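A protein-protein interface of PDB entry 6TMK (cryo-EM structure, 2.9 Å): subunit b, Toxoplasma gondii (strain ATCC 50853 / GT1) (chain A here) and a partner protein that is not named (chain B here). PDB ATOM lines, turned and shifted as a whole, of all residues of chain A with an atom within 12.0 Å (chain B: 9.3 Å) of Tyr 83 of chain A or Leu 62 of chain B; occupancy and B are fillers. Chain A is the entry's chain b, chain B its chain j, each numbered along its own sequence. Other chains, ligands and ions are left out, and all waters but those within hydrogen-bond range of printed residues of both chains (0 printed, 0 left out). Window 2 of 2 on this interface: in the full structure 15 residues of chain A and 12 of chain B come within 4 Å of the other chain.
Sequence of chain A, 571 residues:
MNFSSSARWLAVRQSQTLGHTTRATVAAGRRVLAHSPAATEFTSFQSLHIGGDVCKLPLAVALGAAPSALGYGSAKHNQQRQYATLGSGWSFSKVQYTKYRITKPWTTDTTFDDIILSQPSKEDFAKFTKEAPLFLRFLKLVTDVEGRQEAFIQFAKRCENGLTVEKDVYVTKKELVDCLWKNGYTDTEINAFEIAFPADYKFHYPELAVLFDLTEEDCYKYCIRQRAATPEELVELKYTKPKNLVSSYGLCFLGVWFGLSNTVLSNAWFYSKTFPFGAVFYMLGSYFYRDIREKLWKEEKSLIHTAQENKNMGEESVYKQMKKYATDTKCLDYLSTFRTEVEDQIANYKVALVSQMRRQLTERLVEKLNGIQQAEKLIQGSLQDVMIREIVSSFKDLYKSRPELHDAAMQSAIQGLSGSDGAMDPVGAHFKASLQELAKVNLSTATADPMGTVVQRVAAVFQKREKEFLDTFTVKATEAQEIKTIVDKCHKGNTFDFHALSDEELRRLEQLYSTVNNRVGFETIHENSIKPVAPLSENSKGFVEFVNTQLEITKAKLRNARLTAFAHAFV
The backbone carbonyl oxygen (O) of Ile 58 of chain B lies within hydrogen-bond range of the guanidinium group (NH1) of Arg 225 of chain A.
NE2 of Gln 119 of chain A sits at hydrogen-bond distance from O of Ile 116 of chain A. The side-chain hydroxyl of Tyr 83 of chain A lies within hydrogen-bond range of the side-chain amide nitrogen of Gln 119 of chain A (2.9 Å).
Tyr 83 of chain A touches Leu 59 of chain B. CZ of Tyr 83 of chain A touches CB of Pro 61 of chain B, 3.7 Å away. O of Tyr 83 of chain A touches CD1 of Leu 62 of chain B, at 3.8 Å. Met 55 of chain B touches Ile 115 of chain A. Gln 119 of chain A touches Met 55 of chain B. Pro 120 of chain A touches Met 55 of chain B. Ile 224 of chain A touches Met 55 of chain B. CG2 of Ile 58 of chain B touches CG2 of Ile 224 of chain A, at 3.8 Å. Ala 228 of chain A touches Leu 59 of chain B (CB to CD2, 3.997 Å).
Of the printed residues of chain B, Tyr 83 of chain A touches Leu 59, Pro 61 and Leu 62. No residue of chain B comes within 4 Å of Ala 84 of chain A. Of the printed residues of chain B, Ile 115 of chain A touches Met 55. Of the printed residues of chain B, Pro 120 of chain A touches Met 55 (3.7 Å). Printed residues of chain B within 4 Å of Ala 228 of chain A: Leu 59 (3.997 Å). Of the printed residues of chain A, Met 55 of chain B touches Ile 115, Gln 119, Pro 120 and Ile 224. Gln 60 of chain B touches none of the printed residues of chain A. Leu 62 of chain B touches just one residue of chain A: Tyr 83. No residue of chain A comes within 4 Å of Val 64 of chain B. The nearest residue of chain A that does not touch Leu 62 of chain B is Ala 84 of chain A (4.2 Å).
Of the 20 printed residues of chain A, 7 touch a printed residue of chain B. Hydrophobic or aromatic side chains of chain A that line the printed part of chain B: Tyr 83, Ile 115, Pro 120, Ile 224 and Ala 228. Of the 12 printed residues of chain B, 5 touch a printed residue of chain A. Among the printed residues, no Asp or Glu carboxylate lies within 4 Å of a Lys or Arg side-chain nitrogen of the other chain.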
ATOM      1  N   TYR A  83     -10.985  19.522 -13.969  1.00  0.00           N
ATOM      2  CA  TYR A  83     -11.254  18.921 -15.266  1.00  0.00           C
ATOM      3  C   TYR A  83     -12.193  19.795 -16.077  1.00  0.00           C
ATOM      4  O   TYR A  83     -12.994  20.542 -15.523  1.00  0.00           O
ATOM      5  CB  TYR A  83     -11.847  17.523 -15.095  1.00  0.00           C
ATOM      6  CG  TYR A  83     -10.845  16.501 -14.639  1.00  0.00           C
ATOM      7  CD1 TYR A  83     -10.276  15.618 -15.534  1.00  0.00           C
ATOM      8  CD2 TYR A  83     -10.462  16.423 -13.316  1.00  0.00           C
ATOM      9  CE1 TYR A  83      -9.357  14.690 -15.124  1.00  0.00           C
ATOM     10  CE2 TYR A  83      -9.542  15.498 -12.901  1.00  0.00           C
ATOM     11  CZ  TYR A  83      -8.992  14.636 -13.807  1.00  0.00           C
ATOM     12  OH  TYR A  83      -8.072  13.711 -13.386  1.00  0.00           O
ATOM     13  N   ALA A  84     -12.082  19.700 -17.397  1.00  0.00           N
ATOM     14  CA  ALA A  84     -12.904  20.514 -18.275  1.00  0.00           C
ATOM     15  C   ALA A  84     -14.349  20.040 -18.274  1.00  0.00           C
ATOM     16  O   ALA A  84     -14.645  18.858 -18.080  1.00  0.00           O
ATOM     17  CB  ALA A  84     -12.365  20.482 -19.699  1.00  0.00           C
ATOM     18  N   THR A  85     -15.252  20.986 -18.494  1.00  0.00           N
ATOM     19  CA  THR A  85     -16.679  20.710 -18.611  1.00  0.00           C
ATOM     20  C   THR A  85     -16.995  20.419 -20.071  1.00  0.00           C
ATOM     21  O   THR A  85     -17.163  21.337 -20.876  1.00  0.00           O
ATOM     22  CB  THR A  85     -17.497  21.882 -18.092  1.00  0.00           C
ATOM     23  OG1 THR A  85     -16.979  22.309 -16.829  1.00  0.00           O
ATOM     24  CG2 THR A  85     -18.935  21.491 -17.939  1.00  0.00           C
ATOM     25  N   LEU A  86     -17.080  19.143 -20.415  1.00  0.00           N
ATOM     26  CA  LEU A  86     -17.411  18.748 -21.772  1.00  0.00           C
ATOM     27  C   LEU A  86     -18.923  18.712 -21.963  1.00  0.00           C
ATOM     28  O   LEU A  86     -19.696  18.597 -21.010  1.00  0.00           O
ATOM     29  CB  LEU A  86     -16.814  17.383 -22.099  1.00  0.00           C
ATOM     30  CG  LEU A  86     -15.379  17.158 -21.635  1.00  0.00           C
ATOM     31  CD1 LEU A  86     -14.911  15.776 -22.018  1.00  0.00           C
ATOM     32  CD2 LEU A  86     -14.469  18.210 -22.220  1.00  0.00           C
ATOM     33  N   GLY A  87     -19.332  18.809 -23.217  1.00  0.00           N
ATOM     34  CA  GLY A  87     -20.735  18.818 -23.587  1.00  0.00           C
ATOM     35  C   GLY A  87     -21.024  19.901 -24.606  1.00  0.00           C
ATOM     36  O   GLY A  87     -20.425  20.976 -24.603  1.00  0.00           O
ATOM     37  N   ASP A 114     -18.035   7.257  -9.972  1.00  0.00           N
ATOM     38  CA  ASP A 114     -17.932   8.367 -10.905  1.00  0.00           C
ATOM     39  C   ASP A 114     -16.631   8.268 -11.682  1.00  0.00           C
ATOM     40  O   ASP A 114     -15.575   7.974 -11.120  1.00  0.00           O
ATOM     41  CB  ASP A 114     -18.004   9.695 -10.150  1.00  0.00           C
ATOM     42  CG  ASP A 114     -18.123  10.895 -11.066  1.00  0.00           C
ATOM     43  OD1 ASP A 114     -19.236  11.162 -11.558  1.00  0.00           O
ATOM     44  OD2 ASP A 114     -17.108  11.584 -11.284  1.00  0.00           O
ATOM     45  N   ILE A 115     -16.714   8.514 -12.988  1.00  0.00           N
ATOM     46  CA  ILE A 115     -15.560   8.288 -13.847  1.00  0.00           C
ATOM     47  C   ILE A 115     -14.453   9.288 -13.535  1.00  0.00           C
ATOM     48  O   ILE A 115     -13.268   8.932 -13.507  1.00  0.00           O
ATOM     49  CB  ILE A 115     -15.999   8.335 -15.321  1.00  0.00           C
ATOM     50  CG1 ILE A 115     -14.868   7.895 -16.238  1.00  0.00           C
ATOM     51  CG2 ILE A 115     -16.472   9.714 -15.713  1.00  0.00           C
ATOM     52  CD1 ILE A 115     -15.344   7.528 -17.611  1.00  0.00           C
ATOM     53  N   ILE A 116     -14.815  10.540 -13.260  1.00  0.00           N
ATOM     54  CA  ILE A 116     -13.803  11.560 -13.030  1.00  0.00           C
ATOM     55  C   ILE A 116     -13.163  11.392 -11.661  1.00  0.00           C
ATOM     56  O   ILE A 116     -11.985  11.722 -11.475  1.00  0.00           O
ATOM     57  CB  ILE A 116     -14.427  12.953 -13.206  1.00  0.00           C
ATOM     58  CG1 ILE A 116     -14.597  13.265 -14.686  1.00  0.00           C
ATOM     59  CG2 ILE A 116     -13.580  14.008 -12.550  1.00  0.00           C
ATOM     60  CD1 ILE A 116     -15.732  14.179 -14.984  1.00  0.00           C
ATOM     61  N   LEU A 117     -13.915  10.896 -10.682  1.00  0.00           N
ATOM     62  CA  LEU A 117     -13.363  10.709  -9.350  1.00  0.00           C
ATOM     63  C   LEU A 117     -12.542   9.435  -9.257  1.00  0.00           C
ATOM     64  O   LEU A 117     -11.538   9.400  -8.538  1.00  0.00           O
ATOM     65  CB  LEU A 117     -14.490  10.685  -8.322  1.00  0.00           C
ATOM     66  CG  LEU A 117     -15.241  12.001  -8.149  1.00  0.00           C
ATOM     67  CD1 LEU A 117     -16.480  11.820  -7.314  1.00  0.00           C
ATOM     68  CD2 LEU A 117     -14.345  13.032  -7.526  1.00  0.00           C
ATOM     69  N   SER A 118     -12.954   8.389  -9.969  1.00  0.00           N
ATOM     70  CA  SER A 118     -12.214   7.137  -9.970  1.00  0.00           C
ATOM     71  C   SER A 118     -10.951   7.226 -10.817  1.00  0.00           C
ATOM     72  O   SER A 118      -9.920   6.649 -10.454  1.00  0.00           O
ATOM     73  CB  SER A 118     -13.113   6.018 -10.475  1.00  0.00           C
ATOM     74  OG  SER A 118     -14.023   5.613  -9.476  1.00  0.00           O
ATOM     75  N   GLN A 119     -11.012   7.934 -11.939  1.00  0.00           N
ATOM     76  CA  GLN A 119      -9.958   7.913 -12.946  1.00  0.00           C
ATOM     77  C   GLN A 119      -9.638   6.474 -13.355  1.00  0.00           C
ATOM     78  O   GLN A 119      -8.491   6.031 -13.249  1.00  0.00           O
ATOM     79  CB  GLN A 119      -8.710   8.620 -12.436  1.00  0.00           C
ATOM     80  CG  GLN A 119      -8.872  10.114 -12.263  1.00  0.00           C
ATOM     81  CD  GLN A 119      -9.043  10.822 -13.584  1.00  0.00           C
ATOM     82  OE1 GLN A 119      -8.238  10.657 -14.498  1.00  0.00           O
ATOM     83  NE2 GLN A 119     -10.100  11.611 -13.696  1.00  0.00           N
ATOM     84  N   PRO A 120     -10.629   5.724 -13.826  1.00  0.00           N
ATOM     85  CA  PRO A 120     -10.426   4.292 -14.041  1.00  0.00           C
ATOM     86  C   PRO A 120      -9.591   3.994 -15.270  1.00  0.00           C
ATOM     87  O   PRO A 120      -9.547   4.764 -16.231  1.00  0.00           O
ATOM     88  CB  PRO A 120     -11.851   3.765 -14.204  1.00  0.00           C
ATOM     89  CG  PRO A 120     -12.563   4.884 -14.821  1.00  0.00           C
ATOM     90  CD  PRO A 120     -11.988   6.132 -14.210  1.00  0.00           C
ATOM     91  N   SER A 121      -8.928   2.850 -15.226  1.00  0.00           N
ATOM     92  CA  SER A 121      -8.205   2.311 -16.363  1.00  0.00           C
ATOM     93  C   SER A 121      -8.999   1.181 -17.015  1.00  0.00           C
ATOM     94  O   SER A 121     -10.052   0.747 -16.533  1.00  0.00           O
ATOM     95  CB  SER A 121      -6.819   1.832 -15.939  1.00  0.00           C
ATOM     96  OG  SER A 121      -5.995   2.926 -15.592  1.00  0.00           O
ATOM     97  N   ILE A 224     -14.798   7.262 -24.233  1.00  0.00           N
ATOM     98  CA  ILE A 224     -14.549   7.771 -22.890  1.00  0.00           C
ATOM     99  C   ILE A 224     -14.872   9.253 -22.810  1.00  0.00           C
ATOM    100  O   ILE A 224     -15.470   9.720 -21.835  1.00  0.00           O
ATOM    101  CB  ILE A 224     -13.097   7.492 -22.479  1.00  0.00           C
ATOM    102  CG1 ILE A 224     -12.886   5.996 -22.286  1.00  0.00           C
ATOM    103  CG2 ILE A 224     -12.763   8.232 -21.206  1.00  0.00           C
ATOM    104  CD1 ILE A 224     -13.414   5.467 -21.009  1.00  0.00           C
ATOM    105  N   ARG A 225     -14.476  10.019 -23.826  1.00  0.00           N
ATOM    106  CA  ARG A 225     -14.809  11.437 -23.846  1.00  0.00           C
ATOM    107  C   ARG A 225     -16.319  11.638 -23.861  1.00  0.00           C
ATOM    108  O   ARG A 225     -16.850  12.514 -23.165  1.00  0.00           O
ATOM    109  CB  ARG A 225     -14.167  12.099 -25.060  1.00  0.00           C
ATOM    110  CG  ARG A 225     -12.688  12.387 -24.904  1.00  0.00           C
ATOM    111  CD  ARG A 225     -12.056  12.840 -26.205  1.00  0.00           C
ATOM    112  NE  ARG A 225     -10.815  12.119 -26.473  1.00  0.00           N
ATOM    113  CZ  ARG A 225      -9.599  12.574 -26.195  1.00  0.00           C
ATOM    114  NH1 ARG A 225      -9.427  13.760 -25.640  1.00  0.00           N
ATOM    115  NH2 ARG A 225      -8.544  11.832 -26.473  1.00  0.00           N
ATOM    116  N   ARG A 227     -18.603   9.626 -22.717  1.00  0.00           N
ATOM    117  CA  ARG A 227     -19.173   9.261 -21.425  1.00  0.00           C
ATOM    118  C   ARG A 227     -18.878  10.316 -20.368  1.00  0.00           C
ATOM    119  O   ARG A 227     -19.716  10.581 -19.501  1.00  0.00           O
ATOM    120  CB  ARG A 227     -18.632   7.908 -20.968  1.00  0.00           C
ATOM    121  CG  ARG A 227     -19.116   6.708 -21.764  1.00  0.00           C
ATOM    122  CD  ARG A 227     -20.610   6.578 -21.787  1.00  0.00           C
ATOM    123  NE  ARG A 227     -21.157   7.094 -23.037  1.00  0.00           N
ATOM    124  CZ  ARG A 227     -22.259   7.830 -23.146  1.00  0.00           C
ATOM    125  NH1 ARG A 227     -22.972   8.151 -22.079  1.00  0.00           N
ATOM    126  NH2 ARG A 227     -22.651   8.246 -24.337  1.00  0.00           N
ATOM    127  N   ALA A 228     -17.690  10.916 -20.419  1.00  0.00           N
ATOM    128  CA  ALA A 228     -17.363  12.002 -19.506  1.00  0.00           C
ATOM    129  C   ALA A 228     -18.205  13.238 -19.775  1.00  0.00           C
ATOM    130  O   ALA A 228     -18.417  14.049 -18.868  1.00  0.00           O
ATOM    131  CB  ALA A 228     -15.883  12.340 -19.615  1.00  0.00           C
ATOM    132  N   ALA A 229     -18.670  13.414 -21.010  1.00  0.00           N
ATOM    133  CA  ALA A 229     -19.606  14.497 -21.284  1.00  0.00           C
ATOM    134  C   ALA A 229     -20.881  14.360 -20.462  1.00  0.00           C
ATOM    135  O   ALA A 229     -21.503  15.368 -20.112  1.00  0.00           O
ATOM    136  CB  ALA A 229     -19.944  14.540 -22.769  1.00  0.00           C
ATOM    137  N   THR A 230     -21.285  13.129 -20.145  1.00  0.00           N
ATOM    138  CA  THR A 230     -22.434  12.853 -19.285  1.00  0.00           C
ATOM    139  C   THR A 230     -21.960  12.063 -18.071  1.00  0.00           C
ATOM    140  O   THR A 230     -22.203  10.855 -17.966  1.00  0.00           O
ATOM    141  CB  THR A 230     -23.525  12.085 -20.027  1.00  0.00           C
ATOM    142  OG1 THR A 230     -23.102  10.734 -20.241  1.00  0.00           O
ATOM    143  CG2 THR A 230     -23.837  12.736 -21.358  1.00  0.00           C
ATOM    144  N   PRO A 231     -21.287  12.720 -17.129  1.00  0.00           N
ATOM    145  CA  PRO A 231     -20.729  12.014 -15.975  1.00  0.00           C
ATOM    146  C   PRO A 231     -21.688  11.822 -14.814  1.00  0.00           C
ATOM    147  O   PRO A 231     -21.294  11.239 -13.799  1.00  0.00           O
ATOM    148  CB  PRO A 231     -19.567  12.931 -15.582  1.00  0.00           C
ATOM    149  CG  PRO A 231     -19.960  14.302 -16.077  1.00  0.00           C
ATOM    150  CD  PRO A 231     -21.158  14.172 -16.962  1.00  0.00           C
ATOM    151  N   MET B  55      -6.380   6.997 -17.849  1.00  0.00           N
ATOM    152  CA  MET B  55      -7.295   8.099 -18.086  1.00  0.00           C
ATOM    153  C   MET B  55      -6.578   9.426 -18.261  1.00  0.00           C
ATOM    154  O   MET B  55      -7.182  10.375 -18.764  1.00  0.00           O
ATOM    155  CB  MET B  55      -8.291   8.197 -16.935  1.00  0.00           C
ATOM    156  CG  MET B  55      -9.399   9.195 -17.149  1.00  0.00           C
ATOM    157  SD  MET B  55     -10.404   8.812 -18.583  1.00  0.00           S
ATOM    158  CE  MET B  55     -11.523   7.649 -17.830  1.00  0.00           C
ATOM    159  N   LYS B  56      -5.315   9.528 -17.844  1.00  0.00           N
ATOM    160  CA  LYS B  56      -4.587  10.771 -18.047  1.00  0.00           C
ATOM    161  C   LYS B  56      -4.225  10.991 -19.506  1.00  0.00           C
ATOM    162  O   LYS B  56      -3.939  12.127 -19.896  1.00  0.00           O
ATOM    163  CB  LYS B  56      -3.328  10.792 -17.186  1.00  0.00           C
ATOM    164  CG  LYS B  56      -2.294   9.765 -17.553  1.00  0.00           C
ATOM    165  CD  LYS B  56      -1.159   9.753 -16.551  1.00  0.00           C
ATOM    166  CE  LYS B  56      -0.229   8.575 -16.777  1.00  0.00           C
ATOM    167  NZ  LYS B  56       1.017   8.661 -15.961  1.00  0.00           N
ATOM    168  N   GLU B  57      -4.224   9.937 -20.318  1.00  0.00           N
ATOM    169  CA  GLU B  57      -4.040  10.088 -21.752  1.00  0.00           C
ATOM    170  C   GLU B  57      -5.283  10.614 -22.454  1.00  0.00           C
ATOM    171  O   GLU B  57      -5.223  10.893 -23.655  1.00  0.00           O
ATOM    172  CB  GLU B  57      -3.641   8.749 -22.370  1.00  0.00           C
ATOM    173  CG  GLU B  57      -2.350   8.181 -21.829  1.00  0.00           C
ATOM    174  CD  GLU B  57      -1.894   6.956 -22.589  1.00  0.00           C
ATOM    175  OE1 GLU B  57      -2.612   6.533 -23.520  1.00  0.00           O
ATOM    176  OE2 GLU B  57      -0.820   6.413 -22.258  1.00  0.00           O
ATOM    177  N   ILE B  58      -6.399  10.752 -21.744  1.00  0.00           N
ATOM    178  CA  ILE B  58      -7.671  11.093 -22.364  1.00  0.00           C
ATOM    179  C   ILE B  58      -8.199  12.380 -21.753  1.00  0.00           C
ATOM    180  O   ILE B  58      -8.412  13.376 -22.451  1.00  0.00           O
ATOM    181  CB  ILE B  58      -8.685   9.953 -22.197  1.00  0.00           C
ATOM    182  CG1 ILE B  58      -8.204   8.705 -22.919  1.00  0.00           C
ATOM    183  CG2 ILE B  58     -10.013  10.357 -22.761  1.00  0.00           C
ATOM    184  CD1 ILE B  58      -8.663   7.444 -22.292  1.00  0.00           C
ATOM    185  N   LEU B  59      -8.424  12.357 -20.444  1.00  0.00           N
ATOM    186  CA  LEU B  59      -8.962  13.491 -19.710  1.00  0.00           C
ATOM    187  C   LEU B  59      -7.812  14.209 -19.018  1.00  0.00           C
ATOM    188  O   LEU B  59      -7.177  13.654 -18.117  1.00  0.00           O
ATOM    189  CB  LEU B  59      -9.999  13.029 -18.692  1.00  0.00           C
ATOM    190  CG  LEU B  59     -11.198  12.244 -19.208  1.00  0.00           C
ATOM    191  CD1 LEU B  59     -12.074  11.821 -18.060  1.00  0.00           C
ATOM    192  CD2 LEU B  59     -11.994  13.060 -20.192  1.00  0.00           C
ATOM    193  N   GLN B  60      -7.548  15.430 -19.438  1.00  0.00           N
ATOM    194  CA  GLN B  60      -6.517  16.248 -18.824  1.00  0.00           C
ATOM    195  C   GLN B  60      -7.144  17.157 -17.785  1.00  0.00           C
ATOM    196  O   GLN B  60      -8.125  17.845 -18.095  1.00  0.00           O
ATOM    197  CB  GLN B  60      -5.796  17.083 -19.875  1.00  0.00           C
ATOM    198  CG  GLN B  60      -5.226  16.282 -21.018  1.00  0.00           C
ATOM    199  CD  GLN B  60      -4.091  15.384 -20.593  1.00  0.00           C
ATOM    200  OE1 GLN B  60      -3.293  15.738 -19.725  1.00  0.00           O
ATOM    201  NE2 GLN B  60      -4.008  14.212 -21.205  1.00  0.00           N
ATOM    202  N   PRO B  61      -6.640  17.204 -16.558  1.00  0.00           N
ATOM    203  CA  PRO B  61      -7.205  18.127 -15.578  1.00  0.00           C
ATOM    204  C   PRO B  61      -6.703  19.546 -15.764  1.00  0.00           C
ATOM    205  O   PRO B  61      -5.569  19.791 -16.180  1.00  0.00           O
ATOM    206  CB  PRO B  61      -6.731  17.546 -14.243  1.00  0.00           C
ATOM    207  CG  PRO B  61      -5.478  16.896 -14.570  1.00  0.00           C
ATOM    208  CD  PRO B  61      -5.620  16.340 -15.945  1.00  0.00           C
ATOM    209  N   LEU B  62      -7.582  20.486 -15.451  1.00  0.00           N
ATOM    210  CA  LEU B  62      -7.213  21.885 -15.460  1.00  0.00           C
ATOM    211  C   LEU B  62      -6.242  22.190 -14.327  1.00  0.00           C
ATOM    212  O   LEU B  62      -6.167  21.479 -13.322  1.00  0.00           O
ATOM    213  CB  LEU B  62      -8.451  22.763 -15.320  1.00  0.00           C
ATOM    214  CG  LEU B  62      -9.424  22.825 -16.484  1.00  0.00           C
ATOM    215  CD1 LEU B  62     -10.651  23.533 -16.024  1.00  0.00           C
ATOM    216  CD2 LEU B  62      -8.826  23.553 -17.667  1.00  0.00           C
ATOM    217  N   TRP B  63      -5.491  23.268 -14.504  1.00  0.00           N
ATOM    218  CA  TRP B  63      -4.565  23.744 -13.489  1.00  0.00           C
ATOM    219  C   TRP B  63      -5.278  24.767 -12.618  1.00  0.00           C
ATOM    220  O   TRP B  63      -5.709  25.815 -13.109  1.00  0.00           O
ATOM    221  CB  TRP B  63      -3.315  24.347 -14.122  1.00  0.00           C
ATOM    222  CG  TRP B  63      -2.114  24.247 -13.263  1.00  0.00           C
ATOM    223  CD1 TRP B  63      -1.499  25.271 -12.621  1.00  0.00           C
ATOM    224  CD2 TRP B  63      -1.382  23.066 -12.927  1.00  0.00           C
ATOM    225  NE1 TRP B  63      -0.427  24.810 -11.909  1.00  0.00           N
ATOM    226  CE2 TRP B  63      -0.333  23.455 -12.080  1.00  0.00           C
ATOM    227  CE3 TRP B  63      -1.508  21.718 -13.263  1.00  0.00           C
ATOM    228  CZ2 TRP B  63       0.581  22.553 -11.565  1.00  0.00           C
ATOM    229  CZ3 TRP B  63      -0.599  20.824 -12.749  1.00  0.00           C
ATOM    230  CH2 TRP B  63       0.431  21.243 -11.911  1.00  0.00           C
ATOM    231  N   VAL B  64      -5.414  24.454 -11.329  1.00  0.00           N
ATOM    232  CA  VAL B  64      -6.155  25.294 -10.401  1.00  0.00           C
ATOM    233  C   VAL B  64      -5.396  25.552  -9.109  1.00  0.00           C
ATOM    234  O   VAL B  64      -5.874  26.311  -8.268  1.00  0.00           O
ATOM    235  CB  VAL B  64      -7.543  24.694 -10.094  1.00  0.00           C
ATOM    236  CG1 VAL B  64      -8.309  24.462 -11.367  1.00  0.00           C
ATOM    237  CG2 VAL B  64      -7.422  23.400  -9.344  1.00  0.00           C
ATOM    238  N   VAL B  65      -4.220  24.953  -8.928  1.00  0.00           N
ATOM    239  CA  VAL B  65      -3.495  25.105  -7.671  1.00  0.00           C
ATOM    240  C   VAL B  65      -2.964  26.521  -7.542  1.00  0.00           C
ATOM    241  O   VAL B  65      -3.033  27.135  -6.472  1.00  0.00           O
ATOM    242  CB  VAL B  65      -2.365  24.068  -7.575  1.00  0.00           C
ATOM    243  CG1 VAL B  65      -1.504  24.345  -6.376  1.00  0.00           C
ATOM    244  CG2 VAL B  65      -2.949  22.714  -7.448  1.00  0.00           C
ATOM    245  N   GLU B  66      -2.413  27.052  -8.623  1.00  0.00           N
ATOM    246  CA  GLU B  66      -1.929  28.410  -8.677  1.00  0.00           C
ATOM    247  C   GLU B  66      -2.820  29.203  -9.611  1.00  0.00           C
ATOM    248  O   GLU B  66      -3.122  28.728 -10.713  1.00  0.00           O
ATOM    249  CB  GLU B  66      -0.479  28.456  -9.160  1.00  0.00           C
ATOM    250  CG  GLU B  66      -0.260  27.889 -10.535  1.00  0.00           C
ATOM    251  CD  GLU B  66       1.166  27.431 -10.755  1.00  0.00           C
ATOM    252  OE1 GLU B  66       1.695  26.698  -9.895  1.00  0.00           O
ATOM    253  OE2 GLU B  66       1.759  27.806 -11.787  1.00  0.00           O
